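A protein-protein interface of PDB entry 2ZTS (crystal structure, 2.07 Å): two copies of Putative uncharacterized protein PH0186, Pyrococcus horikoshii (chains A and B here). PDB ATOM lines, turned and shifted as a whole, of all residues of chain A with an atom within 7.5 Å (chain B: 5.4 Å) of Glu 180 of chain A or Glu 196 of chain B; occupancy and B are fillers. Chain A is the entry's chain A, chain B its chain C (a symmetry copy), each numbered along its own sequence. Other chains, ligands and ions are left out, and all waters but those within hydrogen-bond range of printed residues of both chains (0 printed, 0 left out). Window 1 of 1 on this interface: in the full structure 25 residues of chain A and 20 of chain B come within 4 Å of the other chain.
Positions printed for both chains: 34, 188, 189, 190 and 195.
Leu 35 of chain A touches none of the printed residues of chain B.
Of the printed residues of chain B, Thr 39 of chain A touches Leu 189 and Glu 196.
Lys 43 of chain A touches none of the printed residues of chain B.
Of chain B, only Glu 196 and Phe 197 come within 4 Å of Glu 180 of chain A.
Printed residues of chain B within 4 Å of Arg 191 of chain A: Gly 193 (2.9 Å) and Phe 197 (3.9 Å).
Printed residues of chain A within 4 Å of Gly 193 of chain B: Arg 191.
Of chain A, only Thr 39 (3.7 Å) and Glu 180 (3.9 Å) come within 4 Å of Glu 196 of chain B.
The nearest residue of chain A that does not touch Glu 196 of chain B is Arg 191 of chain A (5.4 Å).
The nearest printed residue of chain B that does not touch Pro 145 of chain A is Gly 193 of chain B (6.9 Å).
NH1 of Arg 191 of chain A lies within hydrogen-bond range of O of Gly 193 of chain B (2.9 Å).
Printed residues of chain A that touch a printed residue of chain B: Thr 39, Glu 68, Pro 145, Glu 180 and Arg 191.
Of the 13 printed residues of chain B, 4 touch a printed residue of chain A.
Hydrophobic or aromatic side chains of chain B that line the printed part of chain A: Leu 189 and Phe 197.
Thr 39 of chain A touches Leu 189 of chain B.
Thr 39 of chain A touches Glu 196 of chain B.
Phe 197 of chain B touches Glu 68 of chain A (CD1 to OE1, 3.4 Å).
Phe 197 of chain B touches Pro 145 of chain A.
OE2 of Glu 180 of chain A touches CG of Glu 196 of chain B, 3.9 Å away.
Phe 197 of chain B touches Glu 180 of chain A (CZ to OE2, 3.6 Å).
Arg 191 of chain A touches Phe 197 of chain B (NH1 to CE2, 3.9 Å).
The side-chain carboxylate of Glu 195 of chain A lies within hydrogen-bond range of the backbone NH of Arg 191 of chain A (3.2 Å).
OE1 of Glu 196 of chain B is in hydrogen-bond range of N of Ile 194 of chain B, at 3.5 Å.
OE1 of Glu 195 of chain B lies within hydrogen-bond range of N of Gly 193 of chain B (3.3 Å).
OG1 of Thr 39 of chain A lies within hydrogen-bond range of OE2 of Glu 180 of chain A, at 2.6 Å.
OE1 of Glu 180 of chain A lies within salt-bridge range of NZ of Lys 43 of chain A, 2.6 Å away.
OG of Ser 190 of chain B lies within hydrogen-bond range of OE1 of Glu 196 of chain B, at 2.6 Å.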
ATOM      1  N   LEU A  34      -1.421   9.738 -25.623  1.00  0.00           N
ATOM      2  CA  LEU A  34      -1.821   8.438 -25.215  1.00  0.00           C
ATOM      3  C   LEU A  34      -0.640   7.590 -24.903  1.00  0.00           C
ATOM      4  O   LEU A  34       0.209   7.378 -25.743  1.00  0.00           O
ATOM      5  CB  LEU A  34      -2.627   7.780 -26.313  1.00  0.00           C
ATOM      6  CG  LEU A  34      -3.260   6.541 -25.734  1.00  0.00           C
ATOM      7  CD1 LEU A  34      -4.329   6.910 -24.632  1.00  0.00           C
ATOM      8  CD2 LEU A  34      -3.828   5.728 -26.850  1.00  0.00           C
ATOM      9  N   LEU A  35      -0.599   7.089 -23.676  1.00  0.00           N
ATOM     10  CA  LEU A  35       0.451   6.214 -23.219  1.00  0.00           C
ATOM     11  C   LEU A  35      -0.146   4.844 -22.977  1.00  0.00           C
ATOM     12  O   LEU A  35      -1.023   4.706 -22.115  1.00  0.00           O
ATOM     13  CB  LEU A  35       1.028   6.757 -21.931  1.00  0.00           C
ATOM     14  CG  LEU A  35       2.133   5.952 -21.263  1.00  0.00           C
ATOM     15  CD1 LEU A  35       3.371   5.891 -22.128  1.00  0.00           C
ATOM     16  CD2 LEU A  35       2.512   6.583 -19.932  1.00  0.00           C
ATOM     17  N   THR A  36       0.269   3.881 -23.788  1.00  0.00           N
ATOM     18  CA  THR A  36      -0.396   2.583 -23.910  1.00  0.00           C
ATOM     19  C   THR A  36       0.611   1.449 -23.732  1.00  0.00           C
ATOM     20  O   THR A  36       1.772   1.533 -24.106  1.00  0.00           O
ATOM     21  CB  THR A  36      -1.196   2.459 -25.242  1.00  0.00           C
ATOM     22  OG1 THR A  36      -1.960   1.235 -25.265  1.00  0.00           O
ATOM     23  CG2 THR A  36      -0.294   2.379 -26.513  1.00  0.00           C
ATOM     24  N   GLY A  37       0.150   0.383 -23.123  1.00  0.00           N
ATOM     25  CA  GLY A  37       1.005  -0.714 -22.811  1.00  0.00           C
ATOM     26  C   GLY A  37       0.289  -1.654 -21.908  1.00  0.00           C
ATOM     27  O   GLY A  37      -0.678  -1.250 -21.291  1.00  0.00           O
ATOM     28  N   GLY A  38       0.786  -2.882 -21.859  1.00  0.00           N
ATOM     29  CA  GLY A  38       0.223  -3.923 -21.014  1.00  0.00           C
ATOM     30  C   GLY A  38       0.489  -3.671 -19.533  1.00  0.00           C
ATOM     31  O   GLY A  38       1.251  -2.751 -19.123  1.00  0.00           O
ATOM     32  N   THR A  39      -0.100  -4.527 -18.732  1.00  0.00           N
ATOM     33  CA  THR A  39       0.035  -4.443 -17.302  1.00  0.00           C
ATOM     34  C   THR A  39       1.518  -4.474 -16.974  1.00  0.00           C
ATOM     35  O   THR A  39       2.251  -5.281 -17.492  1.00  0.00           O
ATOM     36  CB  THR A  39      -0.707  -5.610 -16.634  1.00  0.00           C
ATOM     37  OG1 THR A  39      -2.103  -5.610 -17.054  1.00  0.00           O
ATOM     38  CG2 THR A  39      -0.723  -5.423 -15.102  1.00  0.00           C
ATOM     39  N   GLY A  40       1.973  -3.583 -16.111  1.00  0.00           N
ATOM     40  CA  GLY A  40       3.331  -3.631 -15.610  1.00  0.00           C
ATOM     41  C   GLY A  40       4.387  -3.176 -16.586  1.00  0.00           C
ATOM     42  O   GLY A  40       5.543  -3.554 -16.392  1.00  0.00           O
ATOM     43  N   THR A  41       4.027  -2.442 -17.654  1.00  0.00           N
ATOM     44  CA  THR A  41       5.010  -1.997 -18.670  1.00  0.00           C
ATOM     45  C   THR A  41       5.646  -0.659 -18.293  1.00  0.00           C
ATOM     46  O   THR A  41       6.620  -0.248 -18.908  1.00  0.00           O
ATOM     47  CB  THR A  41       4.434  -1.898 -20.077  1.00  0.00           C
ATOM     48  OG1 THR A  41       3.190  -1.168 -20.105  1.00  0.00           O
ATOM     49  CG2 THR A  41       4.082  -3.285 -20.650  1.00  0.00           C
ATOM     50  N   LYS A  43       3.624   2.358 -17.166  1.00  0.00           N
ATOM     51  CA  LYS A  43       2.791   3.485 -17.492  1.00  0.00           C
ATOM     52  C   LYS A  43       2.541   4.467 -16.392  1.00  0.00           C
ATOM     53  O   LYS A  43       2.592   5.681 -16.594  1.00  0.00           O
ATOM     54  CB  LYS A  43       1.435   3.001 -17.982  1.00  0.00           C
ATOM     55  CG  LYS A  43       1.496   2.083 -19.228  1.00  0.00           C
ATOM     56  CD  LYS A  43       0.110   1.752 -19.732  1.00  0.00           C
ATOM     57  CE  LYS A  43      -0.797   1.036 -18.724  1.00  0.00           C
ATOM     58  NZ  LYS A  43      -0.319  -0.351 -18.365  1.00  0.00           N
ATOM     59  N   THR A  44       2.140   3.945 -15.247  1.00  0.00           N
ATOM     60  CA  THR A  44       1.918   4.766 -14.078  1.00  0.00           C
ATOM     61  C   THR A  44       3.210   5.457 -13.663  1.00  0.00           C
ATOM     62  O   THR A  44       3.190   6.627 -13.350  1.00  0.00           O
ATOM     63  CB  THR A  44       1.335   3.914 -12.928  1.00  0.00           C
ATOM     64  OG1 THR A  44      -0.003   3.583 -13.284  1.00  0.00           O
ATOM     65  CG2 THR A  44       1.189   4.716 -11.588  1.00  0.00           C
ATOM     66  N   GLU A  68      -7.011   4.507 -10.446  1.00  0.00           N
ATOM     67  CA  GLU A  68      -6.415   3.166 -10.342  1.00  0.00           C
ATOM     68  C   GLU A  68      -6.099   2.844  -8.882  1.00  0.00           C
ATOM     69  O   GLU A  68      -6.157   1.698  -8.451  1.00  0.00           O
ATOM     70  CB  GLU A  68      -5.124   3.071 -11.160  1.00  0.00           C
ATOM     71  CG  GLU A  68      -5.325   3.070 -12.687  1.00  0.00           C
ATOM     72  CD  GLU A  68      -5.271   1.698 -13.397  1.00  0.00           C
ATOM     73  OE1 GLU A  68      -5.728   1.608 -14.555  1.00  0.00           O
ATOM     74  OE2 GLU A  68      -4.755   0.723 -12.834  1.00  0.00           O
ATOM     75  N   ASP A 142      -4.745   8.604 -15.188  1.00  0.00           N
ATOM     76  CA  ASP A 142      -4.337   7.242 -15.080  1.00  0.00           C
ATOM     77  C   ASP A 142      -5.477   6.541 -14.350  1.00  0.00           C
ATOM     78  O   ASP A 142      -5.538   6.652 -13.111  1.00  0.00           O
ATOM     79  CB  ASP A 142      -3.044   7.172 -14.268  1.00  0.00           C
ATOM     80  CG  ASP A 142      -2.442   5.795 -14.260  1.00  0.00           C
ATOM     81  OD1 ASP A 142      -1.714   5.472 -13.275  1.00  0.00           O
ATOM     82  OD2 ASP A 142      -2.638   4.967 -15.225  1.00  0.00           O
ATOM     83  N   SER A 143      -6.399   5.848 -15.032  1.00  0.00           N
ATOM     84  CA  SER A 143      -6.374   5.502 -16.462  1.00  0.00           C
ATOM     85  C   SER A 143      -7.735   5.545 -17.098  1.00  0.00           C
ATOM     86  O   SER A 143      -8.752   5.685 -16.421  1.00  0.00           O
ATOM     87  CB  SER A 143      -5.856   4.075 -16.601  1.00  0.00           C
ATOM     88  OG  SER A 143      -6.794   3.147 -16.054  1.00  0.00           O
ATOM     89  N   ILE A 144      -7.758   5.536 -18.420  1.00  0.00           N
ATOM     90  CA  ILE A 144      -9.016   5.399 -19.171  1.00  0.00           C
ATOM     91  C   ILE A 144      -9.781   4.150 -18.804  1.00  0.00           C
ATOM     92  O   ILE A 144     -10.998   4.217 -18.553  1.00  0.00           O
ATOM     93  CB  ILE A 144      -8.751   5.515 -20.684  1.00  0.00           C
ATOM     94  CG1 ILE A 144      -8.381   6.950 -20.993  1.00  0.00           C
ATOM     95  CG2 ILE A 144      -9.968   5.128 -21.539  1.00  0.00           C
ATOM     96  CD1 ILE A 144      -7.727   7.119 -22.283  1.00  0.00           C
ATOM     97  N   PRO A 145      -9.147   2.978 -18.798  1.00  0.00           N
ATOM     98  CA  PRO A 145      -9.881   1.789 -18.347  1.00  0.00           C
ATOM     99  C   PRO A 145     -10.487   1.950 -16.930  1.00  0.00           C
ATOM    100  O   PRO A 145     -11.642   1.532 -16.695  1.00  0.00           O
ATOM    101  CB  PRO A 145      -8.835   0.667 -18.386  1.00  0.00           C
ATOM    102  CG  PRO A 145      -7.782   1.179 -19.370  1.00  0.00           C
ATOM    103  CD  PRO A 145      -7.789   2.664 -19.258  1.00  0.00           C
ATOM    104  N   THR A 178      -3.345   7.439 -19.861  1.00  0.00           N
ATOM    105  CA  THR A 178      -2.908   6.060 -19.977  1.00  0.00           C
ATOM    106  C   THR A 178      -4.031   5.092 -20.368  1.00  0.00           C
ATOM    107  O   THR A 178      -5.140   5.278 -19.940  1.00  0.00           O
ATOM    108  CB  THR A 178      -2.250   5.575 -18.706  1.00  0.00           C
ATOM    109  OG1 THR A 178      -3.247   5.435 -17.693  1.00  0.00           O
ATOM    110  CG2 THR A 178      -1.199   6.582 -18.215  1.00  0.00           C
ATOM    111  N   THR A 179      -3.736   4.098 -21.201  1.00  0.00           N
ATOM    112  CA  THR A 179      -4.649   2.995 -21.443  1.00  0.00           C
ATOM    113  C   THR A 179      -3.866   1.707 -21.541  1.00  0.00           C
ATOM    114  O   THR A 179      -2.648   1.706 -21.563  1.00  0.00           O
ATOM    115  CB  THR A 179      -5.494   3.262 -22.665  1.00  0.00           C
ATOM    116  OG1 THR A 179      -6.614   2.359 -22.678  1.00  0.00           O
ATOM    117  CG2 THR A 179      -4.713   3.036 -23.995  1.00  0.00           C
ATOM    118  N   GLU A 180      -4.563   0.600 -21.488  1.00  0.00           N
ATOM    119  CA  GLU A 180      -3.940  -0.690 -21.280  1.00  0.00           C
ATOM    120  C   GLU A 180      -4.603  -1.748 -22.183  1.00  0.00           C
ATOM    121  O   GLU A 180      -5.734  -2.126 -21.945  1.00  0.00           O
ATOM    122  CB  GLU A 180      -4.079  -1.086 -19.793  1.00  0.00           C
ATOM    123  CG  GLU A 180      -3.407  -2.426 -19.403  1.00  0.00           C
ATOM    124  CD  GLU A 180      -3.127  -2.545 -17.905  1.00  0.00           C
ATOM    125  OE1 GLU A 180      -2.387  -1.645 -17.330  1.00  0.00           O
ATOM    126  OE2 GLU A 180      -3.634  -3.550 -17.305  1.00  0.00           O
ATOM    127  N   ALA A 181      -3.887  -2.186 -23.193  1.00  0.00           N
ATOM    128  CA  ALA A 181      -4.185  -3.381 -24.000  1.00  0.00           C
ATOM    129  C   ALA A 181      -2.958  -4.339 -24.077  1.00  0.00           C
ATOM    130  O   ALA A 181      -1.792  -3.873 -24.099  1.00  0.00           O
ATOM    131  CB  ALA A 181      -4.500  -2.975 -25.391  1.00  0.00           C
ATOM    132  N   PRO A 182      -3.206  -5.658 -24.094  1.00  0.00           N
ATOM    133  CA  PRO A 182      -2.153  -6.672 -24.375  1.00  0.00           C
ATOM    134  C   PRO A 182      -1.072  -6.259 -25.397  1.00  0.00           C
ATOM    135  O   PRO A 182       0.103  -6.431 -25.050  1.00  0.00           O
ATOM    136  CB  PRO A 182      -2.968  -7.883 -24.908  1.00  0.00           C
ATOM    137  CG  PRO A 182      -4.298  -7.855 -24.066  1.00  0.00           C
ATOM    138  CD  PRO A 182      -4.498  -6.306 -23.729  1.00  0.00           C
ATOM    139  N   LYS A 188      -3.895  -4.737 -30.939  1.00  0.00           N
ATOM    140  CA  LYS A 188      -4.625  -3.487 -30.659  1.00  0.00           C
ATOM    141  C   LYS A 188      -3.752  -2.446 -29.902  1.00  0.00           C
ATOM    142  O   LYS A 188      -3.084  -2.761 -28.927  1.00  0.00           O
ATOM    143  CB  LYS A 188      -5.984  -3.755 -29.955  1.00  0.00           C
ATOM    144  CG  LYS A 188      -5.893  -4.228 -28.469  1.00  0.00           C
ATOM    145  CD  LYS A 188      -7.212  -4.919 -27.965  1.00  0.00           C
ATOM    146  CE  LYS A 188      -6.916  -6.105 -26.979  1.00  0.00           C
ATOM    147  NZ  LYS A 188      -6.467  -7.412 -27.593  1.00  0.00           N
ATOM    148  N   LEU A 189      -3.775  -1.209 -30.401  1.00  0.00           N
ATOM    149  CA  LEU A 189      -3.081  -0.102 -29.752  1.00  0.00           C
ATOM    150  C   LEU A 189      -3.675   0.342 -28.422  1.00  0.00           C
ATOM    151  O   LEU A 189      -2.954   0.882 -27.557  1.00  0.00           O
ATOM    152  CB  LEU A 189      -3.111   1.088 -30.690  1.00  0.00           C
ATOM    153  CG  LEU A 189      -2.003   2.105 -30.453  1.00  0.00           C
ATOM    154  CD1 LEU A 189      -0.652   1.451 -30.721  1.00  0.00           C
ATOM    155  CD2 LEU A 189      -2.224   3.316 -31.370  1.00  0.00           C
ATOM    156  N   SER A 190      -4.989   0.163 -28.284  1.00  0.00           N
ATOM    157  CA  SER A 190      -5.739   0.592 -27.084  1.00  0.00           C
ATOM    158  C   SER A 190      -6.766  -0.463 -26.639  1.00  0.00           C
ATOM    159  O   SER A 190      -7.046  -1.417 -27.347  1.00  0.00           O
ATOM    160  CB  SER A 190      -6.440   1.897 -27.335  1.00  0.00           C
ATOM    161  OG  SER A 190      -7.384   1.752 -28.409  1.00  0.00           O
ATOM    162  N   ARG A 191      -7.307  -0.280 -25.450  1.00  0.00           N
ATOM    163  CA  ARG A 191      -8.262  -1.210 -24.882  1.00  0.00           C
ATOM    164  C   ARG A 191      -9.562  -1.123 -25.628  1.00  0.00           C
ATOM    165  O   ARG A 191     -10.108  -2.148 -25.964  1.00  0.00           O
ATOM    166  CB  ARG A 191      -8.503  -0.912 -23.414  1.00  0.00           C
ATOM    167  CG  ARG A 191      -9.520  -1.801 -22.751  1.00  0.00           C
ATOM    168  CD  ARG A 191      -9.383  -1.806 -21.239  1.00  0.00           C
ATOM    169  NE  ARG A 191     -10.582  -2.381 -20.612  1.00  0.00           N
ATOM    170  CZ  ARG A 191     -10.686  -3.631 -20.118  1.00  0.00           C
ATOM    171  NH1 ARG A 191      -9.670  -4.492 -20.147  1.00  0.00           N
ATOM    172  NH2 ARG A 191     -11.843  -4.000 -19.580  1.00  0.00           N
ATOM    173  N   TYR A 192     -10.051   0.087 -25.919  1.00  0.00           N
ATOM    174  CA  TYR A 192     -11.399   0.244 -26.539  1.00  0.00           C
ATOM    175  C   TYR A 192     -11.417   0.600 -28.049  1.00  0.00           C
ATOM    176  O   TYR A 192     -12.472   0.581 -28.658  1.00  0.00           O
ATOM    177  CB  TYR A 192     -12.247   1.283 -25.746  1.00  0.00           C
ATOM    178  CG  TYR A 192     -12.438   0.864 -24.276  1.00  0.00           C
ATOM    179  CD1 TYR A 192     -13.236  -0.233 -23.937  1.00  0.00           C
ATOM    180  CD2 TYR A 192     -11.715   1.483 -23.258  1.00  0.00           C
ATOM    181  CE1 TYR A 192     -13.343  -0.682 -22.572  1.00  0.00           C
ATOM    182  CE2 TYR A 192     -11.847   1.093 -21.936  1.00  0.00           C
ATOM    183  CZ  TYR A 192     -12.669   0.039 -21.596  1.00  0.00           C
ATOM    184  OH  TYR A 192     -12.712  -0.330 -20.282  1.00  0.00           O
ATOM    185  N   GLU A 195      -9.469   5.614 -27.713  1.00  0.00           N
ATOM    186  CA  GLU A 195      -8.580   6.517 -26.982  1.00  0.00           C
ATOM    187  C   GLU A 195      -7.700   7.307 -27.943  1.00  0.00           C
ATOM    188  O   GLU A 195      -7.481   8.510 -27.755  1.00  0.00           O
ATOM    189  CB  GLU A 195      -7.690   5.679 -26.019  1.00  0.00           C
ATOM    190  CG  GLU A 195      -8.443   4.915 -24.925  1.00  0.00           C
ATOM    191  CD  GLU A 195      -8.855   3.474 -25.276  1.00  0.00           C
ATOM    192  OE1 GLU A 195      -9.530   3.247 -26.326  1.00  0.00           O
ATOM    193  OE2 GLU A 195      -8.468   2.530 -24.544  1.00  0.00           O
ATOM    194  N   LEU B  34      -2.276 -10.617  -7.962  1.00  0.00           N
ATOM    195  CA  LEU B  34      -3.023 -11.450  -8.866  1.00  0.00           C
ATOM    196  C   LEU B  34      -2.107 -12.570  -9.261  1.00  0.00           C
ATOM    197  O   LEU B  34      -1.041 -12.367  -9.851  1.00  0.00           O
ATOM    198  CB  LEU B  34      -3.471 -10.673 -10.108  1.00  0.00           C
ATOM    199  CG  LEU B  34      -4.434 -11.475 -10.996  1.00  0.00           C
ATOM    200  CD1 LEU B  34      -5.804 -11.709 -10.338  1.00  0.00           C
ATOM    201  CD2 LEU B  34      -4.607 -10.845 -12.346  1.00  0.00           C
ATOM    202  N   LYS B 188      -4.251 -13.272 -23.254  1.00  0.00           N
ATOM    203  CA  LYS B 188      -4.941 -12.758 -22.045  1.00  0.00           C
ATOM    204  C   LYS B 188      -4.162 -13.014 -20.706  1.00  0.00           C
ATOM    205  O   LYS B 188      -3.754 -14.113 -20.408  1.00  0.00           O
ATOM    206  CB  LYS B 188      -6.394 -13.282 -21.956  1.00  0.00           C
ATOM    207  CG  LYS B 188      -7.429 -12.419 -22.654  1.00  0.00           C
ATOM    208  CD  LYS B 188      -8.750 -12.269 -21.848  1.00  0.00           C
ATOM    209  CE  LYS B 188      -8.888 -10.886 -21.129  1.00  0.00           C
ATOM    210  NZ  LYS B 188      -7.910 -10.654 -19.962  1.00  0.00           N
ATOM    211  N   LEU B 189      -3.993 -11.977 -19.902  1.00  0.00           N
ATOM    212  CA  LEU B 189      -3.417 -12.156 -18.561  1.00  0.00           C
ATOM    213  C   LEU B 189      -4.424 -12.793 -17.586  1.00  0.00           C
ATOM    214  O   LEU B 189      -4.063 -13.537 -16.668  1.00  0.00           O
ATOM    215  CB  LEU B 189      -3.062 -10.797 -18.029  1.00  0.00           C
ATOM    216  CG  LEU B 189      -2.007 -10.744 -16.981  1.00  0.00           C
ATOM    217  CD1 LEU B 189      -0.713 -11.424 -17.494  1.00  0.00           C
ATOM    218  CD2 LEU B 189      -1.805  -9.227 -16.658  1.00  0.00           C
ATOM    219  N   SER B 190      -5.690 -12.468 -17.778  1.00  0.00           N
ATOM    220  CA  SER B 190      -6.749 -12.914 -16.884  1.00  0.00           C
ATOM    221  C   SER B 190      -7.981 -13.397 -17.643  1.00  0.00           C
ATOM    222  O   SER B 190      -8.079 -13.217 -18.819  1.00  0.00           O
ATOM    223  CB  SER B 190      -7.166 -11.738 -16.050  1.00  0.00           C
ATOM    224  OG  SER B 190      -7.640 -10.707 -16.890  1.00  0.00           O
ATOM    225  N   GLY B 193     -10.317  -9.700 -17.962  1.00  0.00           N
ATOM    226  CA  GLY B 193      -9.679  -8.450 -18.424  1.00  0.00           C
ATOM    227  C   GLY B 193      -9.798  -7.327 -17.428  1.00  0.00           C
ATOM    228  O   GLY B 193      -9.553  -6.164 -17.773  1.00  0.00           O
ATOM    229  N   ILE B 194     -10.174  -7.663 -16.198  1.00  0.00           N
ATOM    230  CA  ILE B 194     -10.510  -6.663 -15.163  1.00  0.00           C
ATOM    231  C   ILE B 194      -9.657  -6.898 -13.897  1.00  0.00           C
ATOM    232  O   ILE B 194      -9.303  -5.977 -13.198  1.00  0.00           O
ATOM    233  CB  ILE B 194     -12.015  -6.766 -14.830  1.00  0.00           C
ATOM    234  CG1 ILE B 194     -12.882  -6.536 -16.092  1.00  0.00           C
ATOM    235  CG2 ILE B 194     -12.378  -5.807 -13.788  1.00  0.00           C
ATOM    236  CD1 ILE B 194     -14.371  -6.918 -15.933  1.00  0.00           C
ATOM    237  N   GLU B 195      -9.415  -8.170 -13.588  1.00  0.00           N
ATOM    238  CA  GLU B 195      -8.782  -8.572 -12.371  1.00  0.00           C
ATOM    239  C   GLU B 195      -7.475  -7.796 -12.116  1.00  0.00           C
ATOM    240  O   GLU B 195      -7.173  -7.458 -10.970  1.00  0.00           O
ATOM    241  CB  GLU B 195      -8.488 -10.077 -12.428  1.00  0.00           C
ATOM    242  CG  GLU B 195      -9.716 -10.952 -12.491  1.00  0.00           C
ATOM    243  CD  GLU B 195     -10.087 -11.388 -13.915  1.00  0.00           C
ATOM    244  OE1 GLU B 195     -10.382 -10.502 -14.735  1.00  0.00           O
ATOM    245  OE2 GLU B 195     -10.004 -12.613 -14.201  1.00  0.00           O
ATOM    246  N   GLU B 196      -6.656  -7.629 -13.157  1.00  0.00           N
ATOM    247  CA  GLU B 196      -5.369  -6.909 -13.052  1.00  0.00           C
ATOM    248  C   GLU B 196      -5.491  -5.421 -12.655  1.00  0.00           C
ATOM    249  O   GLU B 196      -4.540  -4.848 -12.107  1.00  0.00           O
ATOM    250  CB  GLU B 196      -4.611  -7.013 -14.380  1.00  0.00           C
ATOM    251  CG  GLU B 196      -5.406  -6.525 -15.573  1.00  0.00           C
ATOM    252  CD  GLU B 196      -6.108  -7.629 -16.369  1.00  0.00           C
ATOM    253  OE1 GLU B 196      -6.804  -8.507 -15.809  1.00  0.00           O
ATOM    254  OE2 GLU B 196      -6.053  -7.564 -17.582  1.00  0.00           O
ATOM    255  N   PHE B 197      -6.639  -4.794 -12.912  1.00  0.00           N
ATOM    256  CA  PHE B 197      -6.878  -3.434 -12.454  1.00  0.00           C
ATOM    257  C   PHE B 197      -7.102  -3.256 -10.935  1.00  0.00           C
ATOM    258  O   PHE B 197      -7.223  -2.117 -10.493  1.00  0.00           O
ATOM    259  CB  PHE B 197      -8.029  -2.786 -13.235  1.00  0.00           C
ATOM    260  CG  PHE B 197      -7.718  -2.633 -14.675  1.00  0.00           C
ATOM    261  CD1 PHE B 197      -6.966  -1.553 -15.112  1.00  0.00           C
ATOM    262  CD2 PHE B 197      -8.060  -3.629 -15.571  1.00  0.00           C
ATOM    263  CE1 PHE B 197      -6.620  -1.446 -16.419  1.00  0.00           C
ATOM    264  CE2 PHE B 197      -7.730  -3.517 -16.890  1.00  0.00           C
ATOM    265  CZ  PHE B 197      -7.011  -2.448 -17.326  1.00  0.00           C
ATOM    266  N   ILE B 198      -7.266  -4.341 -10.168  1.00  0.00           N
ATOM    267  CA  ILE B 198      -7.339  -4.201  -8.708  1.00  0.00           C
ATOM    268  C   ILE B 198      -6.132  -4.810  -8.016  1.00  0.00           C
ATOM    269  O   ILE B 198      -6.135  -5.015  -6.838  1.00  0.00           O
ATOM    270  CB  ILE B 198      -8.673  -4.764  -8.148  1.00  0.00           C
ATOM    271  CG1 ILE B 198      -8.766  -6.269  -8.286  1.00  0.00           C
ATOM    272  CG2 ILE B 198      -9.881  -4.072  -8.844  1.00  0.00           C
ATOM    273  CD1 ILE B 198      -9.818  -6.896  -7.376  1.00  0.00           C
ATOM    274  N   ALA B 199      -5.082  -5.094  -8.766  1.00  0.00           N
ATOM    275  CA  ALA B 199      -3.902  -5.728  -8.195  1.00  0.00           C
ATOM    276  C   ALA B 199      -2.665  -4.899  -8.501  1.00  0.00           C
ATOM    277  O   ALA B 199      -2.582  -4.283  -9.551  1.00  0.00           O
ATOM    278  CB  ALA B 199      -3.752  -7.126  -8.737  1.00  0.00           C
ATOM    279  N   ARG B 200      -1.761  -4.807  -7.536  1.00  0.00           N
ATOM    280  CA  ARG B 200      -0.532  -4.044  -7.683  1.00  0.00           C
ATOM    281  C   ARG B 200       0.659  -4.972  -7.880  1.00  0.00           C
ATOM    282  O   ARG B 200       1.797  -4.517  -7.990  1.00  0.00           O
ATOM    283  CB  ARG B 200      -0.305  -3.126  -6.451  1.00  0.00           C
ATOM    284  CG  ARG B 200      -1.533  -2.320  -6.001  1.00  0.00           C
ATOM    285  CD  ARG B 200      -1.850  -1.006  -6.768  1.00  0.00           C
ATOM    286  NE  ARG B 200      -3.144  -0.439  -6.304  1.00  0.00           N
ATOM    287  CZ  ARG B 200      -3.351   0.216  -5.130  1.00  0.00           C
ATOM    288  NH1 ARG B 200      -2.360   0.397  -4.261  1.00  0.00           N
ATOM    289  NH2 ARG B 200      -4.561   0.693  -4.816  1.00  0.00           N
ATOM    290  N   VAL B 202       1.443  -8.894 -10.147  1.00  0.00           N
ATOM    291  CA  VAL B 202       0.956 -10.024 -10.971  1.00  0.00           C
ATOM    292  C   VAL B 202       2.012 -11.106 -11.142  1.00  0.00           C
ATOM    293  O   VAL B 202       3.152 -10.816 -11.532  1.00  0.00           O
ATOM    294  CB  VAL B 202       0.535  -9.565 -12.373  1.00  0.00           C
ATOM    295  CG1 VAL B 202       0.072 -10.733 -13.209  1.00  0.00           C
ATOM    296  CG2 VAL B 202      -0.511  -8.494 -12.265  1.00  0.00           C
